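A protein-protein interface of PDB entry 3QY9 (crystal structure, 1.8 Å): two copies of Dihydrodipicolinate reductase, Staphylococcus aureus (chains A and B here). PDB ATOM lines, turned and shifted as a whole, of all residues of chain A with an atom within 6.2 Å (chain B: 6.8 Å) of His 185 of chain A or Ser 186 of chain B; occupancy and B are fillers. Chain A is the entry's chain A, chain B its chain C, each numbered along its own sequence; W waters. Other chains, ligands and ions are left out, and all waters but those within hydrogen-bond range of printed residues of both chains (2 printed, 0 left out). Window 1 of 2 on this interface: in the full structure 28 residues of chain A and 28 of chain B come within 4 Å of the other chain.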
ATOM      1  N   GLU A 133       9.353 -19.449 -22.318  1.00  0.00           N
ATOM      2  CA  GLU A 133       9.236 -18.424 -21.288  1.00  0.00           C
ATOM      3  C   GLU A 133       7.770 -18.312 -20.883  1.00  0.00           C
ATOM      4  O   GLU A 133       6.888 -18.297 -21.737  1.00  0.00           O
ATOM      5  CB  GLU A 133       9.743 -17.087 -21.819  1.00  0.00           C
ATOM      6  CG  GLU A 133      11.228 -17.096 -22.175  1.00  0.00           C
ATOM      7  CD  GLU A 133      12.120 -16.815 -20.994  1.00  0.00           C
ATOM      8  OE1 GLU A 133      12.051 -15.689 -20.453  1.00  0.00           O
ATOM      9  OE2 GLU A 133      12.919 -17.701 -20.620  1.00  0.00           O
ATOM     10  N   LEU A 134       7.510 -18.264 -19.578  1.00  0.00           N
ATOM     11  CA  LEU A 134       6.142 -18.177 -19.087  1.00  0.00           C
ATOM     12  C   LEU A 134       5.927 -16.828 -18.442  1.00  0.00           C
ATOM     13  O   LEU A 134       6.691 -16.415 -17.560  1.00  0.00           O
ATOM     14  CB  LEU A 134       5.857 -19.287 -18.059  1.00  0.00           C
ATOM     15  CG  LEU A 134       5.968 -20.731 -18.559  1.00  0.00           C
ATOM     16  CD1 LEU A 134       5.975 -21.692 -17.378  1.00  0.00           C
ATOM     17  CD2 LEU A 134       4.826 -21.058 -19.496  1.00  0.00           C
ATOM     18  N   THR A 135       4.874 -16.146 -18.871  1.00  0.00           N
ATOM     19  CA  THR A 135       4.525 -14.866 -18.281  1.00  0.00           C
ATOM     20  C   THR A 135       3.094 -14.916 -17.761  1.00  0.00           C
ATOM     21  O   THR A 135       2.217 -15.499 -18.396  1.00  0.00           O
ATOM     22  CB  THR A 135       4.694 -13.717 -19.308  1.00  0.00           C
ATOM     23  OG1 THR A 135       6.057 -13.657 -19.738  1.00  0.00           O
ATOM     24  CG2 THR A 135       4.312 -12.366 -18.691  1.00  0.00           C
ATOM     25  N   GLU A 136       2.858 -14.315 -16.596  1.00  0.00           N
ATOM     26  CA  GLU A 136       1.495 -14.157 -16.113  1.00  0.00           C
ATOM     27  C   GLU A 136       1.303 -12.746 -15.593  1.00  0.00           C
ATOM     28  O   GLU A 136       2.244 -12.139 -15.096  1.00  0.00           O
ATOM     29  CB  GLU A 136       1.127 -15.215 -15.056  1.00  0.00           C
ATOM     30  CG  GLU A 136       2.046 -15.302 -13.829  1.00  0.00           C
ATOM     31  CD  GLU A 136       1.643 -14.400 -12.662  1.00  0.00           C
ATOM     32  OE1 GLU A 136       0.663 -13.611 -12.761  1.00  0.00           O
ATOM     33  OE2 GLU A 136       2.329 -14.483 -11.627  1.00  0.00           O
ATOM     34  N   ALA A 137       0.091 -12.225 -15.754  1.00  0.00           N
ATOM     35  CA  ALA A 137      -0.245 -10.885 -15.284  1.00  0.00           C
ATOM     36  C   ALA A 137      -1.505 -10.957 -14.452  1.00  0.00           C
ATOM     37  O   ALA A 137      -2.464 -11.624 -14.834  1.00  0.00           O
ATOM     38  CB  ALA A 137      -0.460  -9.934 -16.470  1.00  0.00           C
ATOM     39  N   PRO A 146       4.888 -16.927  -8.704  1.00  0.00           N
ATOM     40  CA  PRO A 146       3.945 -16.787  -9.812  1.00  0.00           C
ATOM     41  C   PRO A 146       2.555 -17.341  -9.463  1.00  0.00           C
ATOM     42  O   PRO A 146       2.376 -17.950  -8.403  1.00  0.00           O
ATOM     43  CB  PRO A 146       4.599 -17.618 -10.922  1.00  0.00           C
ATOM     44  CG  PRO A 146       5.298 -18.713 -10.182  1.00  0.00           C
ATOM     45  CD  PRO A 146       5.812 -18.059  -8.912  1.00  0.00           C
ATOM     46  N   LEU A 150       0.177 -20.392 -13.767  1.00  0.00           N
ATOM     47  CA  LEU A 150       1.521 -20.496 -14.342  1.00  0.00           C
ATOM     48  C   LEU A 150       2.216 -21.771 -13.861  1.00  0.00           C
ATOM     49  O   LEU A 150       2.810 -22.493 -14.666  1.00  0.00           O
ATOM     50  CB  LEU A 150       2.374 -19.246 -14.051  1.00  0.00           C
ATOM     51  CG  LEU A 150       3.745 -19.202 -14.750  1.00  0.00           C
ATOM     52  CD1 LEU A 150       4.189 -17.767 -15.042  1.00  0.00           C
ATOM     53  CD2 LEU A 150       4.830 -19.970 -13.955  1.00  0.00           C
ATOM     54  N   VAL A 167      13.858 -20.093 -14.032  1.00  0.00           N
ATOM     55  CA  VAL A 167      14.709 -18.914 -13.877  1.00  0.00           C
ATOM     56  C   VAL A 167      13.796 -17.722 -13.614  1.00  0.00           C
ATOM     57  O   VAL A 167      12.942 -17.385 -14.439  1.00  0.00           O
ATOM     58  CB  VAL A 167      15.603 -18.677 -15.120  1.00  0.00           C
ATOM     59  CG1 VAL A 167      16.364 -17.359 -15.008  1.00  0.00           C
ATOM     60  CG2 VAL A 167      16.583 -19.842 -15.308  1.00  0.00           C
ATOM     61  N   TYR A 168      13.983 -17.099 -12.455  1.00  0.00           N
ATOM     62  CA  TYR A 168      13.048 -16.087 -11.963  1.00  0.00           C
ATOM     63  C   TYR A 168      13.533 -14.653 -12.065  1.00  0.00           C
ATOM     64  O   TYR A 168      12.717 -13.726 -12.144  1.00  0.00           O
ATOM     65  CB  TYR A 168      12.708 -16.360 -10.502  1.00  0.00           C
ATOM     66  CG  TYR A 168      12.057 -17.690 -10.262  1.00  0.00           C
ATOM     67  CD1 TYR A 168      10.701 -17.879 -10.528  1.00  0.00           C
ATOM     68  CD2 TYR A 168      12.791 -18.762  -9.765  1.00  0.00           C
ATOM     69  CE1 TYR A 168      10.094 -19.104 -10.296  1.00  0.00           C
ATOM     70  CE2 TYR A 168      12.195 -19.986  -9.533  1.00  0.00           C
ATOM     71  CZ  TYR A 168      10.845 -20.147  -9.807  1.00  0.00           C
ATOM     72  OH  TYR A 168      10.245 -21.356  -9.578  1.00  0.00           O
ATOM     73  N   ARG A 170      16.768 -12.499 -13.867  1.00  0.00           N
ATOM     74  CA  ARG A 170      17.998 -12.374 -14.635  1.00  0.00           C
ATOM     75  C   ARG A 170      18.791 -11.121 -14.301  1.00  0.00           C
ATOM     76  O   ARG A 170      19.945 -11.008 -14.700  1.00  0.00           O
ATOM     77  CB  ARG A 170      17.696 -12.436 -16.133  1.00  0.00           C
ATOM     78  CG  ARG A 170      17.224 -13.814 -16.578  1.00  0.00           C
ATOM     79  CD  ARG A 170      16.798 -13.813 -18.029  1.00  0.00           C
ATOM     80  NE  ARG A 170      16.552 -15.178 -18.492  1.00  0.00           N
ATOM     81  CZ  ARG A 170      15.384 -15.646 -18.925  1.00  0.00           C
ATOM     82  NH1 ARG A 170      14.317 -14.856 -19.005  1.00  0.00           N
ATOM     83  NH2 ARG A 170      15.294 -16.920 -19.308  1.00  0.00           N
ATOM     84  N   HIS A 171      18.186 -10.175 -13.575  1.00  0.00           N
ATOM     85  CA  HIS A 171      18.878  -8.937 -13.245  1.00  0.00           C
ATOM     86  C   HIS A 171      20.116  -9.247 -12.414  1.00  0.00           C
ATOM     87  O   HIS A 171      20.016  -9.828 -11.330  1.00  0.00           O
ATOM     88  CB  HIS A 171      17.966  -7.948 -12.502  1.00  0.00           C
ATOM     89  CG  HIS A 171      18.651  -6.679 -12.089  1.00  0.00           C
ATOM     90  ND1 HIS A 171      18.693  -6.247 -10.780  1.00  0.00           N
ATOM     91  CD2 HIS A 171      19.322  -5.749 -12.811  1.00  0.00           C
ATOM     92  CE1 HIS A 171      19.354  -5.106 -10.714  1.00  0.00           C
ATOM     93  NE2 HIS A 171      19.746  -4.781 -11.933  1.00  0.00           N
ATOM     94  N   GLY A 183      12.122 -19.272 -18.226  1.00  0.00           N
ATOM     95  CA  GLY A 183      11.993 -17.975 -17.570  1.00  0.00           C
ATOM     96  C   GLY A 183      10.566 -17.761 -17.113  1.00  0.00           C
ATOM     97  O   GLY A 183       9.625 -18.050 -17.854  1.00  0.00           O
ATOM     98  N   ILE A 184      10.415 -17.257 -15.888  1.00  0.00           N
ATOM     99  CA  ILE A 184       9.108 -17.074 -15.255  1.00  0.00           C
ATOM    100  C   ILE A 184       8.959 -15.603 -14.852  1.00  0.00           C
ATOM    101  O   ILE A 184       9.847 -15.031 -14.221  1.00  0.00           O
ATOM    102  CB  ILE A 184       8.935 -18.041 -14.038  1.00  0.00           C
ATOM    103  CG1 ILE A 184       8.850 -19.499 -14.534  1.00  0.00           C
ATOM    104  CG2 ILE A 184       7.702 -17.667 -13.191  1.00  0.00           C
ATOM    105  CD1 ILE A 184       8.926 -20.558 -13.448  1.00  0.00           C
ATOM    106  N   HIS A 185       7.833 -15.002 -15.236  1.00  0.00           N
ATOM    107  CA  HIS A 185       7.637 -13.560 -15.120  1.00  0.00           C
ATOM    108  C   HIS A 185       6.260 -13.271 -14.561  1.00  0.00           C
ATOM    109  O   HIS A 185       5.273 -13.807 -15.070  1.00  0.00           O
ATOM    110  CB  HIS A 185       7.774 -12.930 -16.509  1.00  0.00           C
ATOM    111  CG  HIS A 185       9.015 -13.354 -17.224  1.00  0.00           C
ATOM    112  ND1 HIS A 185      10.247 -12.793 -16.961  1.00  0.00           N
ATOM    113  CD2 HIS A 185       9.229 -14.318 -18.153  1.00  0.00           C
ATOM    114  CE1 HIS A 185      11.162 -13.376 -17.715  1.00  0.00           C
ATOM    115  NE2 HIS A 185      10.572 -14.305 -18.447  1.00  0.00           N
ATOM    116  N   SER A 186       6.203 -12.438 -13.515  1.00  0.00           N
ATOM    117  CA  SER A 186       4.938 -12.096 -12.878  1.00  0.00           C
ATOM    118  C   SER A 186       4.680 -10.594 -12.916  1.00  0.00           C
ATOM    119  O   SER A 186       5.285  -9.820 -12.177  1.00  0.00           O
ATOM    120  CB  SER A 186       4.884 -12.649 -11.449  1.00  0.00           C
ATOM    121  OG  SER A 186       4.944 -14.072 -11.468  1.00  0.00           O
ATOM    122  N   ILE A 187       3.800 -10.203 -13.829  1.00  0.00           N
ATOM    123  CA  ILE A 187       3.347  -8.825 -13.962  1.00  0.00           C
ATOM    124  C   ILE A 187       2.214  -8.554 -12.972  1.00  0.00           C
ATOM    125  O   ILE A 187       1.265  -9.343 -12.859  1.00  0.00           O
ATOM    126  CB  ILE A 187       2.890  -8.547 -15.420  1.00  0.00           C
ATOM    127  CG1 ILE A 187       4.116  -8.474 -16.341  1.00  0.00           C
ATOM    128  CG2 ILE A 187       1.996  -7.294 -15.497  1.00  0.00           C
ATOM    129  CD1 ILE A 187       3.804  -8.681 -17.811  1.00  0.00           C
ATOM    130  N   LEU B 134       7.435  -2.802 -16.913  1.00  0.00           N
ATOM    131  CA  LEU B 134       8.290  -2.790 -18.093  1.00  0.00           C
ATOM    132  C   LEU B 134       8.739  -4.199 -18.442  1.00  0.00           C
ATOM    133  O   LEU B 134       9.189  -4.952 -17.579  1.00  0.00           O
ATOM    134  CB  LEU B 134       9.526  -1.906 -17.864  1.00  0.00           C
ATOM    135  CG  LEU B 134       9.246  -0.434 -17.557  1.00  0.00           C
ATOM    136  CD1 LEU B 134      10.508   0.268 -17.071  1.00  0.00           C
ATOM    137  CD2 LEU B 134       8.667   0.259 -18.777  1.00  0.00           C
ATOM    138  N   THR B 135       8.592  -4.550 -19.712  1.00  0.00           N
ATOM    139  CA  THR B 135       9.036  -5.851 -20.197  1.00  0.00           C
ATOM    140  C   THR B 135       9.954  -5.647 -21.400  1.00  0.00           C
ATOM    141  O   THR B 135       9.704  -4.795 -22.259  1.00  0.00           O
ATOM    142  CB  THR B 135       7.836  -6.763 -20.565  1.00  0.00           C
ATOM    143  OG1 THR B 135       7.004  -6.956 -19.415  1.00  0.00           O
ATOM    144  CG2 THR B 135       8.316  -8.132 -21.077  1.00  0.00           C
ATOM    145  N   GLU B 136      11.037  -6.412 -21.445  1.00  0.00           N
ATOM    146  CA  GLU B 136      11.851  -6.465 -22.638  1.00  0.00           C
ATOM    147  C   GLU B 136      12.115  -7.918 -22.964  1.00  0.00           C
ATOM    148  O   GLU B 136      12.210  -8.753 -22.062  1.00  0.00           O
ATOM    149  CB  GLU B 136      13.154  -5.660 -22.490  1.00  0.00           C
ATOM    150  CG  GLU B 136      14.014  -5.991 -21.269  1.00  0.00           C
ATOM    151  CD  GLU B 136      15.087  -7.032 -21.543  1.00  0.00           C
ATOM    152  OE1 GLU B 136      15.893  -7.287 -20.629  1.00  0.00           O
ATOM    153  OE2 GLU B 136      15.135  -7.601 -22.656  1.00  0.00           O
ATOM    154  N   ALA B 137      12.189  -8.218 -24.256  1.00  0.00           N
ATOM    155  CA  ALA B 137      12.566  -9.552 -24.705  1.00  0.00           C
ATOM    156  C   ALA B 137      13.736  -9.467 -25.663  1.00  0.00           C
ATOM    157  O   ALA B 137      13.795  -8.570 -26.511  1.00  0.00           O
ATOM    158  CB  ALA B 137      11.390 -10.244 -25.368  1.00  0.00           C
ATOM    159  N   HIS B 138      14.674 -10.397 -25.514  1.00  0.00           N
ATOM    160  CA  HIS B 138      15.836 -10.464 -26.386  1.00  0.00           C
ATOM    161  C   HIS B 138      16.227 -11.904 -26.618  1.00  0.00           C
ATOM    162  O   HIS B 138      15.787 -12.795 -25.894  1.00  0.00           O
ATOM    163  CB  HIS B 138      17.021  -9.672 -25.802  1.00  0.00           C
ATOM    164  CG  HIS B 138      16.865  -8.191 -25.937  1.00  0.00           C
ATOM    165  ND1 HIS B 138      16.112  -7.442 -25.056  1.00  0.00           N
ATOM    166  CD2 HIS B 138      17.328  -7.324 -26.869  1.00  0.00           C
ATOM    167  CE1 HIS B 138      16.118  -6.178 -25.438  1.00  0.00           C
ATOM    168  NE2 HIS B 138      16.853  -6.078 -26.532  1.00  0.00           N
ATOM    169  N   ASP B 144      23.320  -9.613 -20.067  1.00  0.00           N
ATOM    170  CA  ASP B 144      22.884  -8.561 -19.145  1.00  0.00           C
ATOM    171  C   ASP B 144      21.364  -8.450 -19.134  1.00  0.00           C
ATOM    172  O   ASP B 144      20.721  -8.595 -20.174  1.00  0.00           O
ATOM    173  CB  ASP B 144      23.449  -7.197 -19.546  1.00  0.00           C
ATOM    174  CG  ASP B 144      24.957  -7.109 -19.404  1.00  0.00           C
ATOM    175  OD1 ASP B 144      25.582  -8.001 -18.778  1.00  0.00           O
ATOM    176  OD2 ASP B 144      25.511  -6.114 -19.924  1.00  0.00           O
ATOM    177  N   ALA B 145      20.803  -8.185 -17.955  1.00  0.00           N
ATOM    178  CA  ALA B 145      19.378  -7.868 -17.834  1.00  0.00           C
ATOM    179  C   ALA B 145      19.193  -6.813 -16.751  1.00  0.00           C
ATOM    180  O   ALA B 145      19.874  -6.864 -15.726  1.00  0.00           O
ATOM    181  CB  ALA B 145      18.569  -9.117 -17.513  1.00  0.00           C
ATOM    182  N   PRO B 146      18.290  -5.840 -16.979  1.00  0.00           N
ATOM    183  CA  PRO B 146      17.507  -5.652 -18.199  1.00  0.00           C
ATOM    184  C   PRO B 146      18.316  -4.990 -19.313  1.00  0.00           C
ATOM    185  O   PRO B 146      19.466  -4.577 -19.096  1.00  0.00           O
ATOM    186  CB  PRO B 146      16.372  -4.728 -17.737  1.00  0.00           C
ATOM    187  CG  PRO B 146      16.998  -3.900 -16.679  1.00  0.00           C
ATOM    188  CD  PRO B 146      17.987  -4.802 -15.972  1.00  0.00           C
ATOM    189  N   SER B 147      17.723  -4.912 -20.502  1.00  0.00           N
ATOM    190  CA  SER B 147      18.349  -4.242 -21.630  1.00  0.00           C
ATOM    191  C   SER B 147      18.611  -2.764 -21.350  1.00  0.00           C
ATOM    192  O   SER B 147      17.910  -2.137 -20.541  1.00  0.00           O
ATOM    193  CB  SER B 147      17.449  -4.363 -22.855  1.00  0.00           C
ATOM    194  OG  SER B 147      16.271  -3.587 -22.690  1.00  0.00           O
ATOM    195  N   LEU B 150      15.473  -0.790 -22.065  1.00  0.00           N
ATOM    196  CA  LEU B 150      14.528  -0.784 -20.949  1.00  0.00           C
ATOM    197  C   LEU B 150      14.959   0.262 -19.911  1.00  0.00           C
ATOM    198  O   LEU B 150      14.140   1.055 -19.438  1.00  0.00           O
ATOM    199  CB  LEU B 150      14.372  -2.174 -20.310  1.00  0.00           C
ATOM    200  CG  LEU B 150      13.303  -2.270 -19.211  1.00  0.00           C
ATOM    201  CD1 LEU B 150      12.593  -3.635 -19.196  1.00  0.00           C
ATOM    202  CD2 LEU B 150      13.876  -1.929 -17.822  1.00  0.00           C
ATOM    203  N   TYR B 168      12.403  -6.323  -9.536  1.00  0.00           N
ATOM    204  CA  TYR B 168      13.027  -7.213 -10.513  1.00  0.00           C
ATOM    205  C   TYR B 168      12.499  -8.638 -10.525  1.00  0.00           C
ATOM    206  O   TYR B 168      12.622  -9.334 -11.538  1.00  0.00           O
ATOM    207  CB  TYR B 168      14.539  -7.231 -10.302  1.00  0.00           C
ATOM    208  CG  TYR B 168      15.182  -5.909 -10.618  1.00  0.00           C
ATOM    209  CD1 TYR B 168      15.359  -5.500 -11.942  1.00  0.00           C
ATOM    210  CD2 TYR B 168      15.602  -5.057  -9.599  1.00  0.00           C
ATOM    211  CE1 TYR B 168      15.950  -4.283 -12.239  1.00  0.00           C
ATOM    212  CE2 TYR B 168      16.190  -3.832  -9.886  1.00  0.00           C
ATOM    213  CZ  TYR B 168      16.359  -3.454 -11.208  1.00  0.00           C
ATOM    214  OH  TYR B 168      16.943  -2.248 -11.505  1.00  0.00           O
ATOM    215  N   ILE B 184       9.974  -5.036 -13.474  1.00  0.00           N
ATOM    216  CA  ILE B 184      10.929  -5.127 -14.570  1.00  0.00           C
ATOM    217  C   ILE B 184      11.047  -6.602 -14.967  1.00  0.00           C
ATOM    218  O   ILE B 184      11.292  -7.464 -14.122  1.00  0.00           O
ATOM    219  CB  ILE B 184      12.300  -4.525 -14.168  1.00  0.00           C
ATOM    220  CG1 ILE B 184      12.139  -3.028 -13.816  1.00  0.00           C
ATOM    221  CG2 ILE B 184      13.354  -4.754 -15.267  1.00  0.00           C
ATOM    222  CD1 ILE B 184      13.438  -2.312 -13.475  1.00  0.00           C
ATOM    223  N   HIS B 185      10.840  -6.880 -16.252  1.00  0.00           N
ATOM    224  CA  HIS B 185      10.713  -8.252 -16.737  1.00  0.00           C
ATOM    225  C   HIS B 185      11.586  -8.441 -17.968  1.00  0.00           C
ATOM    226  O   HIS B 185      11.432  -7.723 -18.956  1.00  0.00           O
ATOM    227  CB  HIS B 185       9.238  -8.560 -17.053  1.00  0.00           C
ATOM    228  CG  HIS B 185       8.311  -8.211 -15.929  1.00  0.00           C
ATOM    229  ND1 HIS B 185       8.221  -8.966 -14.776  1.00  0.00           N
ATOM    230  CD2 HIS B 185       7.478  -7.159 -15.755  1.00  0.00           C
ATOM    231  CE1 HIS B 185       7.357  -8.401 -13.950  1.00  0.00           C
ATOM    232  NE2 HIS B 185       6.894  -7.304 -14.519  1.00  0.00           N
ATOM    233  N   SER B 186      12.507  -9.402 -17.884  1.00  0.00           N
ATOM    234  CA  SER B 186      13.479  -9.644 -18.942  1.00  0.00           C
ATOM    235  C   SER B 186      13.303 -11.029 -19.535  1.00  0.00           C
ATOM    236  O   SER B 186      13.760 -12.026 -18.962  1.00  0.00           O
ATOM    237  CB  SER B 186      14.908  -9.484 -18.416  1.00  0.00           C
ATOM    238  OG  SER B 186      15.191  -8.130 -18.135  1.00  0.00           O
ATOM    239  N   ILE B 187      12.616 -11.075 -20.678  1.00  0.00           N
ATOM    240  CA  ILE B 187      12.406 -12.317 -21.425  1.00  0.00           C
ATOM    241  C   ILE B 187      13.629 -12.611 -22.296  1.00  0.00           C
ATOM    242  O   ILE B 187      14.157 -11.720 -22.980  1.00  0.00           O
ATOM    243  CB  ILE B 187      11.111 -12.241 -22.266  1.00  0.00           C
ATOM    244  CG1 ILE B 187       9.888 -12.266 -21.335  1.00  0.00           C
ATOM    245  CG2 ILE B 187      11.056 -13.369 -23.329  1.00  0.00           C
ATOM    246  CD1 ILE B 187       8.617 -11.745 -21.964  1.00  0.00           C
ATOM    247  N   ARG B 188      14.089 -13.861 -22.247  1.00  0.00           N
ATOM    248  CA  ARG B 188      15.186 -14.314 -23.092  1.00  0.00           C
ATOM    249  C   ARG B 188      14.742 -15.541 -23.868  1.00  0.00           C
ATOM    250  O   ARG B 188      14.172 -16.470 -23.300  1.00  0.00           O
ATOM    251  CB  ARG B 188      16.438 -14.648 -22.257  1.00  0.00           C
ATOM    252  CG  ARG B 188      17.021 -13.446 -21.474  1.00  0.00           C
ATOM    253  CD  ARG B 188      17.775 -12.498 -22.399  1.00  0.00           C
ATOM    254  NE  ARG B 188      18.236 -11.293 -21.712  1.00  0.00           N
ATOM    255  CZ  ARG B 188      17.549 -10.154 -21.659  1.00  0.00           C
ATOM    256  NH1 ARG B 188      16.344 -10.062 -22.222  1.00  0.00           N
ATOM    257  NH2 ARG B 188      18.052  -9.110 -21.016  1.00  0.00           N
HETATM  258  O   HOH W   1       9.821 -11.024 -14.739  1.00  0.00           O
HETATM  259  O   HOH W   2      11.732 -11.402 -12.928  1.00  0.00           O
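OE1 of Glu 133 of chain A sits at hydrogen-bond distance from N of Arg 188 of chain B (3.3 Å). The backbone carbonyl oxygen (O) of Ser 186 of chain B sits at hydrogen-bond distance from the guanidinium group (NH1) of Arg 170 of chain A. N of Arg 188 of chain B lies close to NH1 of Arg 170 of chain A, 3.4 Å away.
O of Leu 134 of chain A lies within hydrogen-bond range of N of His 185 of chain A. The backbone NH (N) of Glu 136 of chain A lies within hydrogen-bond range of the backbone carbonyl oxygen (O) of His 185 of chain A (2.9 Å). The backbone NH (N) of Ile 187 of chain A is in hydrogen-bond range of the backbone carbonyl oxygen (O) of Glu 136 of chain A (2.8 Å). The side-chain carboxylate (OE1) of Glu 136 of chain B is in hydrogen-bond range of the side-chain hydroxyl (OG) of Ser 186 of chain B (2.7 Å). The side-chain carboxylate (OE2) of Glu 136 of chain B is in salt-bridge range of the guanidinium group (NH1) of Arg 188 of chain B. NH2 of Arg 188 of chain B is in hydrogen-bond range of O of Asp 144 of chain B (2.8 Å).
OE1 of Glu 133 of chain A touches CA of Ile 187 of chain B (3.5 Å). CB of Ala 145 of chain B touches O of Arg 170 of chain A, at 3.7 Å. Ile 187 of chain B touches Arg 170 of chain A (CA to NH1, 3.99 Å). Ala 145 of chain B touches His 171 of chain A. His 171 of chain A touches Pro 146 of chain B (CD2 to CD, 3.6 Å). Tyr 168 of chain B touches His 171 of chain A. Ser 186 of chain B touches His 185 of chain A. Ile 187 of chain B touches His 185 of chain A. His 185 of chain B touches Ser 186 of chain A (CE1 to O, 3.1 Å). Ile 187 of chain A touches His 185 of chain B (CG1 to NE2, 3.5 Å).
Of the printed residues of chain B, His 171 of chain A touches Ala 145, Pro 146 and Tyr 168. His 185 of chain A touches just these residues of chain B: Ser 186 (3.2 Å) and Ile 187 (3.6 Å). Of the printed residues of chain B, Ser 186 of chain A touches His 185 (3.1 Å). Of the printed residues of chain B, Ile 187 of chain A touches Thr 135 (3.97 Å) and His 185 (3.5 Å). Printed residues of chain A within 4 Å of Pro 146 of chain B: His 171. Ser 186 of chain B touches just these residues of chain A: Arg 170 (2.9 Å) and His 185 (3.2 Å). The nearest residue of chain A that does not touch Ser 186 of chain B is Glu 133 of chain A (4.3 Å).
Of the 16 printed residues of chain A, 7 touch a printed residue of chain B. Among the printed residues, 15 pairs touch across the chains.
Thr 135 of chain A touches Ile 187 of chain B, and with the chains exchanged Ile 187 of chain A touches Thr 135 of chain B. His 185 of chain A touches Ser 186 of chain B, and with the chains exchanged Ser 186 of chain A touches His 185 of chain B. His 185 of chain A touches Ile 187 of chain B, and with the chains exchanged Ile 187 of chain A touches His 185 of chain B. Positions printed for both chains: 134, 135, 136, 137, 146, 150, 168, 184, 185, 186 and 187. Of the 15 pairs that touch across the chains among the printed residues, 6 have their exchanged pair printed and touching as well.
Water W1 lies within hydrogen-bond range of a ring nitrogen (ND1) of His 185 of chain B (2.6 Å) and a ring nitrogen (ND1) of His 185 of chain A (2.9 Å). Water W2 lies within hydrogen-bond range of O of Tyr 168 of chain A and O of Tyr 168 of chain B.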
